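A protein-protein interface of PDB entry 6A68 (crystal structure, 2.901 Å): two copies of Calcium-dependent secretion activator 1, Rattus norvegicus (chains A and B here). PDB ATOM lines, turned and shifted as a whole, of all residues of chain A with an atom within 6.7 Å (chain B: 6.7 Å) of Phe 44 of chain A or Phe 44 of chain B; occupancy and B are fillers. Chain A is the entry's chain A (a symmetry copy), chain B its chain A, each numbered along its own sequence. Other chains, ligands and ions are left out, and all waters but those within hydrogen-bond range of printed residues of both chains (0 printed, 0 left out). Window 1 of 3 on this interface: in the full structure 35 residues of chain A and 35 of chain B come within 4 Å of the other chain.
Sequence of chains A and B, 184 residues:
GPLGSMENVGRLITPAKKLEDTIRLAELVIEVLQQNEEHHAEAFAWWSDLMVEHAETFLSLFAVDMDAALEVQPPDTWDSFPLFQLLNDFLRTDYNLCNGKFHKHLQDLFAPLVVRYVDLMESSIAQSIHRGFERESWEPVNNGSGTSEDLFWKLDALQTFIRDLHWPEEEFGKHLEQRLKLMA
His 40 of chain A touches Phe 44 of chain B, and with the chains exchanged Phe 44 of chain A touches His 40 of chain B.
His 40 of chain A touches Ser 48 of chain B, and with the chains exchanged Ser 48 of chain A touches His 40 of chain B.
Ala 43 of chain A touches Trp 47 of chain B, and with the chains exchanged Trp 47 of chain A touches Ala 43 of chain B.
Phe 44 of chain B touches its own counterpart, Phe 44 of chain A.
Of the 9 pairs that touch across the chains among the printed residues, 9 have their exchanged pair printed and touching as well.
Hydrophobic or aromatic side chains of chain B within 4 Å of the printed part of chain A: His 40, Ala 43, Phe 44 and Trp 47.
Of the 12 printed residues of chain A, 5 touch a printed residue of chain B.
Hydrophobic or aromatic side chains of chain A within 4 Å of the printed part of chain B: His 40, Ala 43, Phe 44 and Trp 47.
Along chain A the printed residues that touch a printed residue of chain B span positions 40 to 48.
Among the printed residues, no Asp or Glu carboxylate lies within 4 Å of a Lys or Arg side-chain nitrogen of the other chain.
The backbone carbonyl oxygen of Phe 44 of chain B is in hydrogen-bond range of a ring nitrogen (NE2) of His 40 of chain A, at 3.1 Å.
NE2 of His 40 of chain B sits at hydrogen-bond distance from O of Phe 44 of chain A (3.1 Å).
Among the printed residues, pairs that only touch across the chains: His 40 of chain A with Trp 47 of chain B (3.5 Å), His 40 of chain A with Ser 48 of chain B (3.7 Å), Ala 43 of chain A with Trp 47 of chain B (3.5 Å), Phe 44 of chain A with Phe 44 of chain B (3.1 Å), Trp 47 of chain A with His 40 of chain B (3.5 Å), Trp 47 of chain A with Ala 43 of chain B (3.5 Å) and Ser 48 of chain A with His 40 of chain B (3.7 Å).
Of the printed residues of chain B, His 40 of chain A touches Phe 44 (3.1 Å), Trp 47 (3.5 Å) and Ser 48 (3.7 Å).
Printed residues of chain A within 4 Å of His 40 of chain B: Phe 44, Trp 47 and Ser 48.
Printed residues of chain A within 4 Å of Ala 43 of chain B: Trp 47 (3.5 Å).
Of the printed residues of chain A, Trp 47 of chain B touches His 40 and Ala 43.
The nearest residue of chain B that does not touch Phe 44 of chain A is Trp 47 of chain B (5.6 Å).
The nearest residue of chain A that does not touch Phe 44 of chain B is Trp 47 of chain A (5.6 Å).
The nearest printed residue of chain A that does not touch Ala 43 of chain B is His 40 of chain A (5.3 Å).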
ATOM      1  N   HIS A  39     -19.467 -14.952  -5.492  1.00  0.00           N
ATOM      2  CA  HIS A  39     -20.537 -14.260  -6.201  1.00  0.00           C
ATOM      3  C   HIS A  39     -21.247 -13.265  -5.291  1.00  0.00           C
ATOM      4  O   HIS A  39     -21.414 -12.094  -5.640  1.00  0.00           O
ATOM      5  CB  HIS A  39     -21.523 -15.276  -6.754  1.00  0.00           C
ATOM      6  CG  HIS A  39     -20.963 -16.114  -7.852  1.00  0.00           C
ATOM      7  ND1 HIS A  39     -19.830 -15.759  -8.550  1.00  0.00           N
ATOM      8  CD2 HIS A  39     -21.378 -17.291  -8.374  1.00  0.00           C
ATOM      9  CE1 HIS A  39     -19.574 -16.679  -9.461  1.00  0.00           C
ATOM     10  NE2 HIS A  39     -20.497 -17.621  -9.373  1.00  0.00           N
ATOM     11  N   HIS A  40     -21.662 -13.716  -4.110  1.00  0.00           N
ATOM     12  CA  HIS A  40     -22.381 -12.845  -3.191  1.00  0.00           C
ATOM     13  C   HIS A  40     -21.530 -11.648  -2.806  1.00  0.00           C
ATOM     14  O   HIS A  40     -21.980 -10.504  -2.876  1.00  0.00           O
ATOM     15  CB  HIS A  40     -22.796 -13.646  -1.959  1.00  0.00           C
ATOM     16  CG  HIS A  40     -23.500 -12.847  -0.911  1.00  0.00           C
ATOM     17  ND1 HIS A  40     -22.827 -12.122   0.050  1.00  0.00           N
ATOM     18  CD2 HIS A  40     -24.820 -12.691  -0.645  1.00  0.00           C
ATOM     19  CE1 HIS A  40     -23.705 -11.547   0.855  1.00  0.00           C
ATOM     20  NE2 HIS A  40     -24.920 -11.873   0.454  1.00  0.00           N
ATOM     21  N   ALA A  41     -20.283 -11.887  -2.426  1.00  0.00           N
ATOM     22  CA  ALA A  41     -19.409 -10.774  -2.072  1.00  0.00           C
ATOM     23  C   ALA A  41     -19.274  -9.784  -3.219  1.00  0.00           C
ATOM     24  O   ALA A  41     -19.358  -8.569  -3.017  1.00  0.00           O
ATOM     25  CB  ALA A  41     -18.046 -11.305  -1.655  1.00  0.00           C
ATOM     26  N   GLU A  42     -19.082 -10.286  -4.433  1.00  0.00           N
ATOM     27  CA  GLU A  42     -18.832  -9.411  -5.565  1.00  0.00           C
ATOM     28  C   GLU A  42     -20.056  -8.598  -5.936  1.00  0.00           C
ATOM     29  O   GLU A  42     -19.925  -7.456  -6.377  1.00  0.00           O
ATOM     30  CB  GLU A  42     -18.374 -10.230  -6.761  1.00  0.00           C
ATOM     31  CG  GLU A  42     -17.761  -9.386  -7.833  1.00  0.00           C
ATOM     32  CD  GLU A  42     -17.105 -10.206  -8.902  1.00  0.00           C
ATOM     33  OE1 GLU A  42     -16.663  -9.616  -9.911  1.00  0.00           O
ATOM     34  OE2 GLU A  42     -17.041 -11.442  -8.731  1.00  0.00           O
ATOM     35  N   ALA A  43     -21.247  -9.170  -5.797  1.00  0.00           N
ATOM     36  CA  ALA A  43     -22.450  -8.420  -6.120  1.00  0.00           C
ATOM     37  C   ALA A  43     -22.711  -7.352  -5.072  1.00  0.00           C
ATOM     38  O   ALA A  43     -23.098  -6.231  -5.412  1.00  0.00           O
ATOM     39  CB  ALA A  43     -23.638  -9.369  -6.237  1.00  0.00           C
ATOM     40  N   PHE A  44     -22.531  -7.700  -3.793  1.00  0.00           N
ATOM     41  CA  PHE A  44     -22.563  -6.729  -2.703  1.00  0.00           C
ATOM     42  C   PHE A  44     -21.720  -5.509  -3.044  1.00  0.00           C
ATOM     43  O   PHE A  44     -22.145  -4.366  -2.833  1.00  0.00           O
ATOM     44  CB  PHE A  44     -22.062  -7.397  -1.416  1.00  0.00           C
ATOM     45  CG  PHE A  44     -21.791  -6.448  -0.264  1.00  0.00           C
ATOM     46  CD1 PHE A  44     -20.680  -5.618  -0.249  1.00  0.00           C
ATOM     47  CD2 PHE A  44     -22.625  -6.437   0.833  1.00  0.00           C
ATOM     48  CE1 PHE A  44     -20.445  -4.764   0.813  1.00  0.00           C
ATOM     49  CE2 PHE A  44     -22.386  -5.593   1.902  1.00  0.00           C
ATOM     50  CZ  PHE A  44     -21.301  -4.760   1.891  1.00  0.00           C
ATOM     51  N   ALA A  45     -20.510  -5.736  -3.559  1.00  0.00           N
ATOM     52  CA  ALA A  45     -19.617  -4.623  -3.841  1.00  0.00           C
ATOM     53  C   ALA A  45     -20.160  -3.768  -4.973  1.00  0.00           C
ATOM     54  O   ALA A  45     -20.273  -2.549  -4.839  1.00  0.00           O
ATOM     55  CB  ALA A  45     -18.228  -5.142  -4.178  1.00  0.00           C
ATOM     56  N   TRP A  46     -20.497  -4.395  -6.099  1.00  0.00           N
ATOM     57  CA  TRP A  46     -21.066  -3.676  -7.231  1.00  0.00           C
ATOM     58  C   TRP A  46     -22.219  -2.784  -6.794  1.00  0.00           C
ATOM     59  O   TRP A  46     -22.218  -1.573  -7.038  1.00  0.00           O
ATOM     60  CB  TRP A  46     -21.550  -4.669  -8.275  1.00  0.00           C
ATOM     61  CG  TRP A  46     -20.479  -5.354  -9.008  1.00  0.00           C
ATOM     62  CD1 TRP A  46     -19.203  -4.937  -9.168  1.00  0.00           C
ATOM     63  CD2 TRP A  46     -20.589  -6.599  -9.704  1.00  0.00           C
ATOM     64  NE1 TRP A  46     -18.499  -5.841  -9.929  1.00  0.00           N
ATOM     65  CE2 TRP A  46     -19.331  -6.874 -10.266  1.00  0.00           C
ATOM     66  CE3 TRP A  46     -21.633  -7.508  -9.907  1.00  0.00           C
ATOM     67  CZ2 TRP A  46     -19.086  -8.019 -11.016  1.00  0.00           C
ATOM     68  CZ3 TRP A  46     -21.385  -8.635 -10.656  1.00  0.00           C
ATOM     69  CH2 TRP A  46     -20.122  -8.883 -11.201  1.00  0.00           C
ATOM     70  N   TRP A  47     -23.225  -3.375  -6.154  1.00  0.00           N
ATOM     71  CA  TRP A  47     -24.371  -2.592  -5.717  1.00  0.00           C
ATOM     72  C   TRP A  47     -23.945  -1.525  -4.711  1.00  0.00           C
ATOM     73  O   TRP A  47     -24.448  -0.397  -4.742  1.00  0.00           O
ATOM     74  CB  TRP A  47     -25.432  -3.534  -5.149  1.00  0.00           C
ATOM     75  CG  TRP A  47     -26.744  -2.908  -4.749  1.00  0.00           C
ATOM     76  CD1 TRP A  47     -27.020  -1.583  -4.616  1.00  0.00           C
ATOM     77  CD2 TRP A  47     -27.949  -3.600  -4.405  1.00  0.00           C
ATOM     78  NE1 TRP A  47     -28.313  -1.403  -4.213  1.00  0.00           N
ATOM     79  CE2 TRP A  47     -28.907  -2.629  -4.078  1.00  0.00           C
ATOM     80  CE3 TRP A  47     -28.311  -4.945  -4.356  1.00  0.00           C
ATOM     81  CZ2 TRP A  47     -30.205  -2.959  -3.698  1.00  0.00           C
ATOM     82  CZ3 TRP A  47     -29.595  -5.270  -3.980  1.00  0.00           C
ATOM     83  CH2 TRP A  47     -30.529  -4.280  -3.655  1.00  0.00           C
ATOM     84  N   SER A  48     -22.992  -1.845  -3.836  1.00  0.00           N
ATOM     85  CA  SER A  48     -22.529  -0.855  -2.869  1.00  0.00           C
ATOM     86  C   SER A  48     -21.801   0.289  -3.563  1.00  0.00           C
ATOM     87  O   SER A  48     -22.170   1.454  -3.404  1.00  0.00           O
ATOM     88  CB  SER A  48     -21.627  -1.505  -1.825  1.00  0.00           C
ATOM     89  OG  SER A  48     -21.356  -0.599  -0.771  1.00  0.00           O
ATOM     90  N   ASP A  49     -20.758  -0.024  -4.331  1.00  0.00           N
ATOM     91  CA  ASP A  49     -20.019   1.028  -5.019  1.00  0.00           C
ATOM     92  C   ASP A  49     -20.961   1.957  -5.772  1.00  0.00           C
ATOM     93  O   ASP A  49     -20.788   3.177  -5.752  1.00  0.00           O
ATOM     94  CB  ASP A  49     -18.985   0.433  -5.984  1.00  0.00           C
ATOM     95  CG  ASP A  49     -18.028  -0.533  -5.311  1.00  0.00           C
ATOM     96  OD1 ASP A  49     -17.828  -0.442  -4.078  1.00  0.00           O
ATOM     97  OD2 ASP A  49     -17.469  -1.392  -6.031  1.00  0.00           O
ATOM     98  N   TYR A  95     -21.435   4.405   7.691  1.00  0.00           N
ATOM     99  CA  TYR A  95     -20.179   3.773   7.312  1.00  0.00           C
ATOM    100  C   TYR A  95     -19.727   4.249   5.943  1.00  0.00           C
ATOM    101  O   TYR A  95     -18.546   4.545   5.739  1.00  0.00           O
ATOM    102  CB  TYR A  95     -20.346   2.252   7.346  1.00  0.00           C
ATOM    103  CG  TYR A  95     -19.154   1.467   6.852  1.00  0.00           C
ATOM    104  CD1 TYR A  95     -17.904   1.614   7.446  1.00  0.00           C
ATOM    105  CD2 TYR A  95     -19.282   0.559   5.804  1.00  0.00           C
ATOM    106  CE1 TYR A  95     -16.805   0.893   7.000  1.00  0.00           C
ATOM    107  CE2 TYR A  95     -18.188  -0.169   5.350  1.00  0.00           C
ATOM    108  CZ  TYR A  95     -16.951   0.004   5.954  1.00  0.00           C
ATOM    109  OH  TYR A  95     -15.857  -0.708   5.515  1.00  0.00           O
ATOM    110  N   HIS B  39     -32.304  -1.057   1.753  1.00  0.00           N
ATOM    111  CA  HIS B  39     -32.524  -2.006   0.669  1.00  0.00           C
ATOM    112  C   HIS B  39     -31.308  -2.900   0.462  1.00  0.00           C
ATOM    113  O   HIS B  39     -31.424  -4.127   0.419  1.00  0.00           O
ATOM    114  CB  HIS B  39     -32.854  -1.251  -0.609  1.00  0.00           C
ATOM    115  CG  HIS B  39     -34.177  -0.564  -0.572  1.00  0.00           C
ATOM    116  ND1 HIS B  39     -35.154  -0.889   0.344  1.00  0.00           N
ATOM    117  CD2 HIS B  39     -34.686   0.430  -1.336  1.00  0.00           C
ATOM    118  CE1 HIS B  39     -36.213  -0.127   0.138  1.00  0.00           C
ATOM    119  NE2 HIS B  39     -35.953   0.682  -0.874  1.00  0.00           N
ATOM    120  N   HIS B  40     -30.127  -2.297   0.346  1.00  0.00           N
ATOM    121  CA  HIS B  40     -28.915  -3.070   0.112  1.00  0.00           C
ATOM    122  C   HIS B  40     -28.676  -4.051   1.246  1.00  0.00           C
ATOM    123  O   HIS B  40     -28.440  -5.237   1.016  1.00  0.00           O
ATOM    124  CB  HIS B  40     -27.735  -2.118  -0.053  1.00  0.00           C
ATOM    125  CG  HIS B  40     -26.417  -2.795  -0.248  1.00  0.00           C
ATOM    126  ND1 HIS B  40     -25.642  -3.233   0.806  1.00  0.00           N
ATOM    127  CD2 HIS B  40     -25.716  -3.074  -1.373  1.00  0.00           C
ATOM    128  CE1 HIS B  40     -24.525  -3.760   0.334  1.00  0.00           C
ATOM    129  NE2 HIS B  40     -24.545  -3.679  -0.984  1.00  0.00           N
ATOM    130  N   ALA B  41     -28.760  -3.581   2.484  1.00  0.00           N
ATOM    131  CA  ALA B  41     -28.566  -4.482   3.613  1.00  0.00           C
ATOM    132  C   ALA B  41     -29.553  -5.641   3.579  1.00  0.00           C
ATOM    133  O   ALA B  41     -29.173  -6.798   3.786  1.00  0.00           O
ATOM    134  CB  ALA B  41     -28.695  -3.707   4.915  1.00  0.00           C
ATOM    135  N   GLU B  42     -30.817  -5.352   3.298  1.00  0.00           N
ATOM    136  CA  GLU B  42     -31.841  -6.380   3.354  1.00  0.00           C
ATOM    137  C   GLU B  42     -31.679  -7.404   2.248  1.00  0.00           C
ATOM    138  O   GLU B  42     -31.982  -8.581   2.450  1.00  0.00           O
ATOM    139  CB  GLU B  42     -33.219  -5.745   3.271  1.00  0.00           C
ATOM    140  CG  GLU B  42     -34.311  -6.684   3.677  1.00  0.00           C
ATOM    141  CD  GLU B  42     -35.634  -5.996   3.817  1.00  0.00           C
ATOM    142  OE1 GLU B  42     -36.645  -6.699   4.036  1.00  0.00           O
ATOM    143  OE2 GLU B  42     -35.661  -4.753   3.699  1.00  0.00           O
ATOM    144  N   ALA B  43     -31.235  -6.981   1.070  1.00  0.00           N
ATOM    145  CA  ALA B  43     -31.043  -7.932  -0.013  1.00  0.00           C
ATOM    146  C   ALA B  43     -29.835  -8.812   0.257  1.00  0.00           C
ATOM    147  O   ALA B  43     -29.876 -10.017   0.001  1.00  0.00           O
ATOM    148  CB  ALA B  43     -30.890  -7.188  -1.336  1.00  0.00           C
ATOM    149  N   PHE B  44     -28.744  -8.212   0.745  1.00  0.00           N
ATOM    150  CA  PHE B  44     -27.584  -8.958   1.225  1.00  0.00           C
ATOM    151  C   PHE B  44     -28.016 -10.097   2.137  1.00  0.00           C
ATOM    152  O   PHE B  44     -27.528 -11.227   2.015  1.00  0.00           O
ATOM    153  CB  PHE B  44     -26.634  -8.002   1.957  1.00  0.00           C
ATOM    154  CG  PHE B  44     -25.518  -8.676   2.733  1.00  0.00           C
ATOM    155  CD1 PHE B  44     -25.758  -9.334   3.931  1.00  0.00           C
ATOM    156  CD2 PHE B  44     -24.218  -8.595   2.285  1.00  0.00           C
ATOM    157  CE1 PHE B  44     -24.727  -9.937   4.629  1.00  0.00           C
ATOM    158  CE2 PHE B  44     -23.183  -9.185   2.987  1.00  0.00           C
ATOM    159  CZ  PHE B  44     -23.438  -9.854   4.153  1.00  0.00           C
ATOM    160  N   ALA B  45     -28.925  -9.810   3.071  1.00  0.00           N
ATOM    161  CA  ALA B  45     -29.333 -10.828   4.028  1.00  0.00           C
ATOM    162  C   ALA B  45     -30.099 -11.942   3.338  1.00  0.00           C
ATOM    163  O   ALA B  45     -29.775 -13.118   3.499  1.00  0.00           O
ATOM    164  CB  ALA B  45     -30.173 -10.199   5.130  1.00  0.00           C
ATOM    165  N   TRP B  46     -31.127 -11.586   2.568  1.00  0.00           N
ATOM    166  CA  TRP B  46     -31.902 -12.571   1.828  1.00  0.00           C
ATOM    167  C   TRP B  46     -30.998 -13.513   1.046  1.00  0.00           C
ATOM    168  O   TRP B  46     -31.064 -14.737   1.198  1.00  0.00           O
ATOM    169  CB  TRP B  46     -32.853 -11.863   0.876  1.00  0.00           C
ATOM    170  CG  TRP B  46     -33.981 -11.189   1.530  1.00  0.00           C
ATOM    171  CD1 TRP B  46     -34.493 -11.455   2.752  1.00  0.00           C
ATOM    172  CD2 TRP B  46     -34.762 -10.122   0.986  1.00  0.00           C
ATOM    173  NE1 TRP B  46     -35.556 -10.622   3.014  1.00  0.00           N
ATOM    174  CE2 TRP B  46     -35.736  -9.790   1.943  1.00  0.00           C
ATOM    175  CE3 TRP B  46     -34.731  -9.413  -0.220  1.00  0.00           C
ATOM    176  CZ2 TRP B  46     -36.671  -8.782   1.733  1.00  0.00           C
ATOM    177  CZ3 TRP B  46     -35.663  -8.421  -0.424  1.00  0.00           C
ATOM    178  CH2 TRP B  46     -36.620  -8.114   0.549  1.00  0.00           C
ATOM    179  N   TRP B  47     -30.148 -12.953   0.189  1.00  0.00           N
ATOM    180  CA  TRP B  47     -29.259 -13.787  -0.607  1.00  0.00           C
ATOM    181  C   TRP B  47     -28.316 -14.582   0.293  1.00  0.00           C
ATOM    182  O   TRP B  47     -28.029 -15.753   0.023  1.00  0.00           O
ATOM    183  CB  TRP B  47     -28.506 -12.906  -1.602  1.00  0.00           C
ATOM    184  CG  TRP B  47     -27.618 -13.616  -2.593  1.00  0.00           C
ATOM    185  CD1 TRP B  47     -27.226 -14.918  -2.565  1.00  0.00           C
ATOM    186  CD2 TRP B  47     -26.994 -13.040  -3.745  1.00  0.00           C
ATOM    187  NE1 TRP B  47     -26.402 -15.191  -3.620  1.00  0.00           N
ATOM    188  CE2 TRP B  47     -26.244 -14.051  -4.363  1.00  0.00           C
ATOM    189  CE3 TRP B  47     -27.008 -11.768  -4.319  1.00  0.00           C
ATOM    190  CZ2 TRP B  47     -25.508 -13.833  -5.523  1.00  0.00           C
ATOM    191  CZ3 TRP B  47     -26.280 -11.553  -5.467  1.00  0.00           C
ATOM    192  CH2 TRP B  47     -25.538 -12.583  -6.058  1.00  0.00           C
ATOM    193  N   SER B  48     -27.852 -13.981   1.389  1.00  0.00           N
ATOM    194  CA  SER B  48     -26.967 -14.704   2.296  1.00  0.00           C
ATOM    195  C   SER B  48     -27.702 -15.848   2.980  1.00  0.00           C
ATOM    196  O   SER B  48     -27.277 -17.002   2.899  1.00  0.00           O
ATOM    197  CB  SER B  48     -26.373 -13.757   3.335  1.00  0.00           C
ATOM    198  OG  SER B  48     -25.355 -14.406   4.073  1.00  0.00           O
ATOM    199  N   ASP B  49     -28.804 -15.548   3.666  1.00  0.00           N
ATOM    200  CA  ASP B  49     -29.549 -16.601   4.346  1.00  0.00           C
ATOM    201  C   ASP B  49     -29.821 -17.771   3.411  1.00  0.00           C
ATOM    202  O   ASP B  49     -29.696 -18.932   3.805  1.00  0.00           O
ATOM    203  CB  ASP B  49     -30.870 -16.063   4.912  1.00  0.00           C
ATOM    204  CG  ASP B  49     -30.683 -14.869   5.830  1.00  0.00           C
ATOM    205  OD1 ASP B  49     -29.583 -14.703   6.406  1.00  0.00           O
ATOM    206  OD2 ASP B  49     -31.654 -14.092   5.977  1.00  0.00           O
ATOM    207  N   TYR B  95     -16.746 -17.717   7.476  1.00  0.00           N
ATOM    208  CA  TYR B  95     -17.597 -17.006   8.420  1.00  0.00           C
ATOM    209  C   TYR B  95     -18.961 -17.662   8.518  1.00  0.00           C
ATOM    210  O   TYR B  95     -19.500 -17.831   9.616  1.00  0.00           O
ATOM    211  CB  TYR B  95     -17.714 -15.541   7.992  1.00  0.00           C
ATOM    212  CG  TYR B  95     -18.671 -14.710   8.812  1.00  0.00           C
ATOM    213  CD1 TYR B  95     -18.505 -14.576  10.187  1.00  0.00           C
ATOM    214  CD2 TYR B  95     -19.731 -14.037   8.208  1.00  0.00           C
ATOM    215  CE1 TYR B  95     -19.378 -13.810  10.948  1.00  0.00           C
ATOM    216  CE2 TYR B  95     -20.610 -13.266   8.960  1.00  0.00           C
ATOM    217  CZ  TYR B  95     -20.427 -13.158  10.330  1.00  0.00           C
ATOM    218  OH  TYR B  95     -21.292 -12.399  11.089  1.00  0.00           O
